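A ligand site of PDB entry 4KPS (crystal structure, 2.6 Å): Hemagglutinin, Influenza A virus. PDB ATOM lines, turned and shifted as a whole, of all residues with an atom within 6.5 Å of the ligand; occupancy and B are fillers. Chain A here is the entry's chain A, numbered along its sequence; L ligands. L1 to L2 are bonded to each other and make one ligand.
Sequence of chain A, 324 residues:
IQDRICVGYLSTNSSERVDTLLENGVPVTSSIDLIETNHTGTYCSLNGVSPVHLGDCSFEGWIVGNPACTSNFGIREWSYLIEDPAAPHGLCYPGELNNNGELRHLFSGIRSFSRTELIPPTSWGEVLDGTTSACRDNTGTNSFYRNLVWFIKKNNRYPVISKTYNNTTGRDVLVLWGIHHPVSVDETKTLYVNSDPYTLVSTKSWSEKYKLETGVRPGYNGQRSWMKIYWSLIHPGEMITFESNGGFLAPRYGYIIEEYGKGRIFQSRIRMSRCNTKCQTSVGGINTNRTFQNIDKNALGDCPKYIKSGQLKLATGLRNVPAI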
ATOM      1  N   TYR A  93       0.544   0.696  -3.755  1.00  0.00           N
ATOM      2  CA  TYR A  93       1.793   1.399  -3.508  1.00  0.00           C
ATOM      3  C   TYR A  93       2.001   2.467  -4.583  1.00  0.00           C
ATOM      4  O   TYR A  93       1.820   2.186  -5.769  1.00  0.00           O
ATOM      5  CB  TYR A  93       2.974   0.419  -3.519  1.00  0.00           C
ATOM      6  CG  TYR A  93       4.209   0.971  -2.847  1.00  0.00           C
ATOM      7  CD1 TYR A  93       4.506   0.660  -1.532  1.00  0.00           C
ATOM      8  CD2 TYR A  93       5.088   1.803  -3.536  1.00  0.00           C
ATOM      9  CE1 TYR A  93       5.637   1.151  -0.917  1.00  0.00           C
ATOM     10  CE2 TYR A  93       6.217   2.310  -2.927  1.00  0.00           C
ATOM     11  CZ  TYR A  93       6.489   1.980  -1.618  1.00  0.00           C
ATOM     12  OH  TYR A  93       7.607   2.467  -1.005  1.00  0.00           O
ATOM     13  N   ASP A 129      11.393 -11.467   1.069  1.00  0.00           N
ATOM     14  CA  ASP A 129      10.187 -10.937   0.448  1.00  0.00           C
ATOM     15  C   ASP A 129       9.681  -9.752   1.252  1.00  0.00           C
ATOM     16  O   ASP A 129       9.353  -9.881   2.429  1.00  0.00           O
ATOM     17  CB  ASP A 129       9.106 -12.018   0.367  1.00  0.00           C
ATOM     18  CG  ASP A 129       9.565 -13.250  -0.392  1.00  0.00           C
ATOM     19  OD1 ASP A 129      10.788 -13.428  -0.573  1.00  0.00           O
ATOM     20  OD2 ASP A 129       8.698 -14.043  -0.811  1.00  0.00           O
ATOM     21  N   GLY A 130       9.622  -8.592   0.598  1.00  0.00           N
ATOM     22  CA  GLY A 130       9.218  -7.365   1.264  1.00  0.00           C
ATOM     23  C   GLY A 130       7.740  -7.077   1.140  1.00  0.00           C
ATOM     24  O   GLY A 130       7.146  -7.228   0.074  1.00  0.00           O
ATOM     25  N   THR A 131       7.138  -6.655   2.249  1.00  0.00           N
ATOM     26  CA  THR A 131       5.734  -6.272   2.252  1.00  0.00           C
ATOM     27  C   THR A 131       5.626  -4.799   2.582  1.00  0.00           C
ATOM     28  O   THR A 131       6.639  -4.111   2.706  1.00  0.00           O
ATOM     29  CB  THR A 131       4.937  -7.098   3.273  1.00  0.00           C
ATOM     30  OG1 THR A 131       5.452  -6.857   4.592  1.00  0.00           O
ATOM     31  CG2 THR A 131       5.047  -8.591   2.958  1.00  0.00           C
ATOM     32  N   THR A 132       4.402  -4.301   2.704  1.00  0.00           N
ATOM     33  CA  THR A 132       4.193  -2.893   3.018  1.00  0.00           C
ATOM     34  C   THR A 132       2.790  -2.620   3.553  1.00  0.00           C
ATOM     35  O   THR A 132       1.852  -3.364   3.270  1.00  0.00           O
ATOM     36  CB  THR A 132       4.451  -1.981   1.794  1.00  0.00           C
ATOM     37  OG1 THR A 132       4.183  -0.620   2.143  1.00  0.00           O
ATOM     38  CG2 THR A 132       3.573  -2.383   0.624  1.00  0.00           C
ATOM     39  N   SER A 133       2.668  -1.556   4.343  1.00  0.00           N
ATOM     40  CA  SER A 133       1.384  -1.197   4.943  1.00  0.00           C
ATOM     41  C   SER A 133       0.474  -0.524   3.922  1.00  0.00           C
ATOM     42  O   SER A 133      -0.700  -0.284   4.189  1.00  0.00           O
ATOM     43  CB  SER A 133       1.602  -0.258   6.134  1.00  0.00           C
ATOM     44  OG  SER A 133       2.169   0.973   5.706  1.00  0.00           O
ATOM     45  N   ALA A 134       1.023  -0.229   2.746  1.00  0.00           N
ATOM     46  CA  ALA A 134       0.246   0.365   1.667  1.00  0.00           C
ATOM     47  C   ALA A 134      -0.588  -0.698   0.957  1.00  0.00           C
ATOM     48  O   ALA A 134      -1.638  -0.389   0.393  1.00  0.00           O
ATOM     49  CB  ALA A 134       1.161   1.085   0.695  1.00  0.00           C
ATOM     50  N   ASN A 142       0.298  -6.788   6.519  1.00  0.00           N
ATOM     51  CA  ASN A 142       1.093  -6.204   5.446  1.00  0.00           C
ATOM     52  C   ASN A 142       1.382  -7.223   4.355  1.00  0.00           C
ATOM     53  O   ASN A 142       1.765  -8.355   4.639  1.00  0.00           O
ATOM     54  CB  ASN A 142       2.404  -5.618   5.985  1.00  0.00           C
ATOM     55  CG  ASN A 142       2.188  -4.336   6.753  1.00  0.00           C
ATOM     56  OD1 ASN A 142       1.059  -3.890   6.949  1.00  0.00           O
ATOM     57  ND2 ASN A 142       3.287  -3.724   7.183  1.00  0.00           N
ATOM     58  N   TRP A 150       8.540  -8.434  -4.016  1.00  0.00           N
ATOM     59  CA  TRP A 150       9.461  -7.362  -3.675  1.00  0.00           C
ATOM     60  C   TRP A 150      10.698  -7.915  -2.975  1.00  0.00           C
ATOM     61  O   TRP A 150      10.711  -8.071  -1.755  1.00  0.00           O
ATOM     62  CB  TRP A 150       8.773  -6.340  -2.774  1.00  0.00           C
ATOM     63  CG  TRP A 150       9.526  -5.064  -2.601  1.00  0.00           C
ATOM     64  CD1 TRP A 150      10.794  -4.789  -3.029  1.00  0.00           C
ATOM     65  CD2 TRP A 150       9.061  -3.877  -1.951  1.00  0.00           C
ATOM     66  NE1 TRP A 150      11.148  -3.508  -2.689  1.00  0.00           N
ATOM     67  CE2 TRP A 150      10.102  -2.927  -2.028  1.00  0.00           C
ATOM     68  CE3 TRP A 150       7.861  -3.523  -1.316  1.00  0.00           C
ATOM     69  CZ2 TRP A 150       9.978  -1.641  -1.484  1.00  0.00           C
ATOM     70  CZ3 TRP A 150       7.750  -2.253  -0.787  1.00  0.00           C
ATOM     71  CH2 TRP A 150       8.797  -1.329  -0.872  1.00  0.00           C
ATOM     72  N   ILE A 152      14.290  -8.093  -1.299  1.00  0.00           N
ATOM     73  CA  ILE A 152      15.161  -7.216  -0.519  1.00  0.00           C
ATOM     74  C   ILE A 152      16.363  -7.971   0.044  1.00  0.00           C
ATOM     75  O   ILE A 152      16.485  -9.181  -0.141  1.00  0.00           O
ATOM     76  CB  ILE A 152      14.405  -6.533   0.631  1.00  0.00           C
ATOM     77  CG1 ILE A 152      13.597  -7.561   1.431  1.00  0.00           C
ATOM     78  CG2 ILE A 152      13.488  -5.449   0.091  1.00  0.00           C
ATOM     79  CD1 ILE A 152      12.883  -6.973   2.627  1.00  0.00           C
ATOM     80  N   HIS A 180      11.533  -0.524  -8.289  1.00  0.00           N
ATOM     81  CA  HIS A 180      11.268   0.372  -7.171  1.00  0.00           C
ATOM     82  C   HIS A 180      12.314   1.467  -7.068  1.00  0.00           C
ATOM     83  O   HIS A 180      13.515   1.184  -7.010  1.00  0.00           O
ATOM     84  CB  HIS A 180      11.187  -0.404  -5.853  1.00  0.00           C
ATOM     85  CG  HIS A 180      11.111   0.474  -4.646  1.00  0.00           C
ATOM     86  ND1 HIS A 180      12.099   0.501  -3.678  1.00  0.00           N
ATOM     87  CD2 HIS A 180      10.182   1.381  -4.255  1.00  0.00           C
ATOM     88  CE1 HIS A 180      11.774   1.376  -2.749  1.00  0.00           C
ATOM     89  NE2 HIS A 180      10.621   1.929  -3.067  1.00  0.00           N
ATOM     90  N   HIS A 181      11.850   2.713  -7.059  1.00  0.00           N
ATOM     91  CA  HIS A 181      12.718   3.877  -6.924  1.00  0.00           C
ATOM     92  C   HIS A 181      12.573   4.446  -5.522  1.00  0.00           C
ATOM     93  O   HIS A 181      11.575   5.103  -5.212  1.00  0.00           O
ATOM     94  CB  HIS A 181      12.356   4.931  -7.963  1.00  0.00           C
ATOM     95  CG  HIS A 181      12.287   4.415  -9.361  1.00  0.00           C
ATOM     96  ND1 HIS A 181      13.328   4.551 -10.253  1.00  0.00           N
ATOM     97  CD2 HIS A 181      11.308   3.741 -10.024  1.00  0.00           C
ATOM     98  CE1 HIS A 181      12.991   3.989 -11.409  1.00  0.00           C
ATOM     99  NE2 HIS A 181      11.776   3.497 -11.286  1.00  0.00           N
ATOM    100  N   PRO A 182      13.566   4.192  -4.651  1.00  0.00           N
ATOM    101  CA  PRO A 182      13.534   4.641  -3.258  1.00  0.00           C
ATOM    102  C   PRO A 182      13.571   6.159  -3.116  1.00  0.00           C
ATOM    103  O   PRO A 182      13.842   6.865  -4.089  1.00  0.00           O
ATOM    104  CB  PRO A 182      14.793   4.011  -2.665  1.00  0.00           C
ATOM    105  CG  PRO A 182      15.127   2.874  -3.569  1.00  0.00           C
ATOM    106  CD  PRO A 182      14.737   3.351  -4.934  1.00  0.00           C
ATOM    107  N   VAL A 183      13.314   6.643  -1.904  1.00  0.00           N
ATOM    108  CA  VAL A 183      13.273   8.085  -1.643  1.00  0.00           C
ATOM    109  C   VAL A 183      14.654   8.732  -1.667  1.00  0.00           C
ATOM    110  O   VAL A 183      14.772   9.938  -1.888  1.00  0.00           O
ATOM    111  CB  VAL A 183      12.598   8.395  -0.289  1.00  0.00           C
ATOM    112  CG1 VAL A 183      11.114   8.080  -0.347  1.00  0.00           C
ATOM    113  CG2 VAL A 183      13.275   7.630   0.826  1.00  0.00           C
ATOM    114  N   GLU A 187      17.933   4.997   1.436  1.00  0.00           N
ATOM    115  CA  GLU A 187      16.927   3.951   1.507  1.00  0.00           C
ATOM    116  C   GLU A 187      17.262   2.776   0.601  1.00  0.00           C
ATOM    117  O   GLU A 187      17.007   1.626   0.957  1.00  0.00           O
ATOM    118  CB  GLU A 187      15.536   4.499   1.184  1.00  0.00           C
ATOM    119  CG  GLU A 187      14.604   4.592   2.394  1.00  0.00           C
ATOM    120  CD  GLU A 187      15.178   5.432   3.523  1.00  0.00           C
ATOM    121  OE1 GLU A 187      14.942   5.070   4.697  1.00  0.00           O
ATOM    122  OE2 GLU A 187      15.853   6.442   3.243  1.00  0.00           O
ATOM    123  N   LEU A 191      17.666  -0.976   1.844  1.00  0.00           N
ATOM    124  CA  LEU A 191      16.835  -2.023   1.264  1.00  0.00           C
ATOM    125  C   LEU A 191      17.600  -3.021   0.397  1.00  0.00           C
ATOM    126  O   LEU A 191      17.309  -4.216   0.411  1.00  0.00           O
ATOM    127  CB  LEU A 191      15.694  -1.405   0.444  1.00  0.00           C
ATOM    128  CG  LEU A 191      14.542  -0.770   1.220  1.00  0.00           C
ATOM    129  CD1 LEU A 191      13.604  -0.043   0.277  1.00  0.00           C
ATOM    130  CD2 LEU A 191      13.794  -1.835   2.012  1.00  0.00           C
ATOM    131  N   GLY A 222       0.839   5.733   3.189  1.00  0.00           N
ATOM    132  CA  GLY A 222       2.089   6.068   3.815  1.00  0.00           C
ATOM    133  C   GLY A 222       3.260   6.558   2.987  1.00  0.00           C
ATOM    134  O   GLY A 222       3.957   7.457   3.419  1.00  0.00           O
ATOM    135  N   GLN A 223       3.474   5.976   1.816  1.00  0.00           N
ATOM    136  CA  GLN A 223       4.782   5.896   1.188  1.00  0.00           C
ATOM    137  C   GLN A 223       5.108   7.123   0.367  1.00  0.00           C
ATOM    138  O   GLN A 223       4.228   7.916   0.024  1.00  0.00           O
ATOM    139  CB  GLN A 223       4.873   4.638   0.336  1.00  0.00           C
ATOM    140  CG  GLN A 223       4.603   3.373   1.127  1.00  0.00           C
ATOM    141  CD  GLN A 223       5.321   3.362   2.465  1.00  0.00           C
ATOM    142  OE1 GLN A 223       6.544   3.499   2.527  1.00  0.00           O
ATOM    143  NE2 GLN A 223       4.560   3.202   3.544  1.00  0.00           N
ATOM    144  N   ARG A 224       6.387   7.275   0.060  1.00  0.00           N
ATOM    145  CA  ARG A 224       6.848   8.463  -0.618  1.00  0.00           C
ATOM    146  C   ARG A 224       7.838   8.139  -1.737  1.00  0.00           C
ATOM    147  O   ARG A 224       8.390   9.039  -2.362  1.00  0.00           O
ATOM    148  CB  ARG A 224       7.460   9.427   0.405  1.00  0.00           C
ATOM    149  CG  ARG A 224       7.037  10.845   0.196  1.00  0.00           C
ATOM    150  CD  ARG A 224       6.401  11.455   1.435  1.00  0.00           C
ATOM    151  NE  ARG A 224       5.541  12.547   1.017  1.00  0.00           N
ATOM    152  CZ  ARG A 224       5.992  13.670   0.476  1.00  0.00           C
ATOM    153  NH1 ARG A 224       7.300  13.841   0.312  1.00  0.00           N
ATOM    154  NH2 ARG A 224       5.152  14.630   0.113  1.00  0.00           N
ATOM    155  N   SER A 225       8.063   6.858  -1.980  1.00  0.00           N
ATOM    156  CA  SER A 225       8.899   6.432  -3.088  1.00  0.00           C
ATOM    157  C   SER A 225       8.044   6.157  -4.312  1.00  0.00           C
ATOM    158  O   SER A 225       6.859   6.476  -4.326  1.00  0.00           O
ATOM    159  CB  SER A 225       9.708   5.188  -2.709  1.00  0.00           C
ATOM    160  OG  SER A 225       8.865   4.157  -2.268  1.00  0.00           O
ATOM    161  N   TRP A 226       8.644   5.559  -5.340  1.00  0.00           N
ATOM    162  CA  TRP A 226       7.912   5.334  -6.583  1.00  0.00           C
ATOM    163  C   TRP A 226       8.208   3.984  -7.230  1.00  0.00           C
ATOM    164  O   TRP A 226       9.359   3.570  -7.310  1.00  0.00           O
ATOM    165  CB  TRP A 226       8.191   6.463  -7.572  1.00  0.00           C
ATOM    166  CG  TRP A 226       7.166   6.574  -8.656  1.00  0.00           C
ATOM    167  CD1 TRP A 226       7.341   6.308  -9.984  1.00  0.00           C
ATOM    168  CD2 TRP A 226       5.797   6.943  -8.499  1.00  0.00           C
ATOM    169  NE1 TRP A 226       6.161   6.506 -10.664  1.00  0.00           N
ATOM    170  CE2 TRP A 226       5.198   6.903  -9.772  1.00  0.00           C
ATOM    171  CE3 TRP A 226       5.015   7.324  -7.401  1.00  0.00           C
ATOM    172  CZ2 TRP A 226       3.861   7.228  -9.981  1.00  0.00           C
ATOM    173  CZ3 TRP A 226       3.687   7.644  -7.612  1.00  0.00           C
ATOM    174  CH2 TRP A 226       3.122   7.583  -8.890  1.00  0.00           C
ATOM    175  N   MET A 227       7.158   3.325  -7.693  1.00  0.00           N
ATOM    176  CA  MET A 227       7.299   2.065  -8.416  1.00  0.00           C
ATOM    177  C   MET A 227       6.849   2.211  -9.864  1.00  0.00           C
ATOM    178  O   MET A 227       5.833   2.827 -10.155  1.00  0.00           O
ATOM    179  CB  MET A 227       6.486   0.957  -7.735  1.00  0.00           C
ATOM    180  CG  MET A 227       7.027   0.539  -6.396  1.00  0.00           C
ATOM    181  SD  MET A 227       6.060  -0.780  -5.642  1.00  0.00           S
ATOM    182  CE  MET A 227       7.080  -1.146  -4.206  1.00  0.00           C
HETATM  183  C1  LIG L   1       8.098   5.253   8.162  1.00  0.00           C
HETATM  184  C2  LIG L   1       7.308   4.050   7.632  1.00  0.00           C
HETATM  185  C3  LIG L   1       8.245   2.883   7.257  1.00  0.00           C
HETATM  186  C4  LIG L   1       9.226   3.499   6.278  1.00  0.00           C
HETATM  187  C5  LIG L   1      10.020   4.575   6.989  1.00  0.00           C
HETATM  188  C6  LIG L   1      11.242   5.099   6.216  1.00  0.00           C
HETATM  189  O1  LIG L   1       7.154   6.297   8.332  1.00  0.00           O
HETATM  190  O2  LIG L   1       6.215   3.718   8.503  1.00  0.00           O
HETATM  191  O3  LIG L   1       7.488   1.879   6.590  1.00  0.00           O
HETATM  192  O4  LIG L   1       8.419   4.191   5.332  1.00  0.00           O
HETATM  193  O5  LIG L   1       9.126   5.644   7.243  1.00  0.00           O
HETATM  194  O6  LIG L   1      11.606   6.385   6.704  1.00  0.00           O
HETATM  195  C1  LG2 L   2       6.054   0.486   5.053  1.00  0.00           C
HETATM  196  C2  LG2 L   2       7.360   1.178   5.331  1.00  0.00           C
HETATM  197  C3  LG2 L   2       7.863  -0.084   5.980  1.00  0.00           C
HETATM  198  C4  LG2 L   2       7.855  -1.305   5.103  1.00  0.00           C
HETATM  199  C5  LG2 L   2       8.753  -1.156   4.049  1.00  0.00           C
HETATM  200  C6  LG2 L   2       8.456   0.139   3.381  1.00  0.00           C
HETATM  201  C7  LG2 L   2       9.508   0.443   2.415  1.00  0.00           C
HETATM  202  C8  LG2 L   2       9.338   1.885   1.946  1.00  0.00           C
HETATM  203  C9  LG2 L   2      10.429   2.270   0.997  1.00  0.00           C
HETATM  204  C10 LG2 L   2       9.878  -2.812   2.498  1.00  0.00           C
HETATM  205  C11 LG2 L   2       9.836  -3.951   1.518  1.00  0.00           C
HETATM  206  N1  LG2 L   2       8.666  -2.294   3.078  1.00  0.00           N
HETATM  207  O1  LG2 L   2       5.535  -0.296   5.925  1.00  0.00           O
HETATM  208  O2  LG2 L   2       5.476   0.694   3.962  1.00  0.00           O
HETATM  209  O3  LG2 L   2       8.176  -2.519   5.850  1.00  0.00           O
HETATM  210  O4  LG2 L   2       8.396   1.216   4.409  1.00  0.00           O
HETATM  211  O5  LG2 L   2      10.762   0.233   2.990  1.00  0.00           O
HETATM  212  O6  LG2 L   2       8.147   2.033   1.324  1.00  0.00           O
HETATM  213  O7  LG2 L   2      10.269   3.448   0.300  1.00  0.00           O
HETATM  214  O8  LG2 L   2      10.957  -2.307   2.811  1.00  0.00           O
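An oxygen (O6) of LG2 L2 sits at hydrogen-bond distance from the side-chain hydroxyl of Tyr 93, at 2.4 Å.
OE1 of Gln 223 lies within hydrogen-bond range of O6 of LG2 L2 (2.5 Å).
An oxygen (O2) of LG2 L2 is in hydrogen-bond range of the side-chain hydroxyl (OG1) of Thr 132 (2.6 Å).
O of Thr 131 sits at hydrogen-bond distance from N1 of LG2 L2.
An oxygen (O7) of LG2 L2 sits at hydrogen-bond distance from the side-chain hydroxyl of Ser 225.
OH of Tyr 93 sits at hydrogen-bond distance from OG of Ser 225 (2.5 Å).
The backbone NH (N) of Ala 134 lies close to the side-chain hydroxyl (OG1) of Thr 132 (3.2 Å).
OG of Ser 225 is in hydrogen-bond range of NE2 of His 180 (2.9 Å).
The backbone NH (N) of Gly 130 lies within hydrogen-bond range of the backbone carbonyl oxygen (O) of Trp 150 (2.6 Å).
CA of Gly 130 touches C11 of LG2 L2, at 3.5 Å.
Ser 133 touches the ligand.
CE3 of Trp 150 touches C11 of LG2 L2, at 3.5 Å.
NE2 of His 180 touches O7 of LG2 L2, 3.7 Å away.
OE1 of Glu 187 touches C6 of LIG L1, at 3.9998 Å.
CD2 of Leu 191 touches O8 of LG2 L2, at 3.0 Å.
Hydrophobic or aromatic side chains that line the ligand: Tyr 93, Trp 150, His 180 and Leu 191.
Of the 22 residues printed, 11 come within 4 Å of the ligand.
The nearest printed residue that does not touch the ligand is Ile 152 (4.2 Å).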
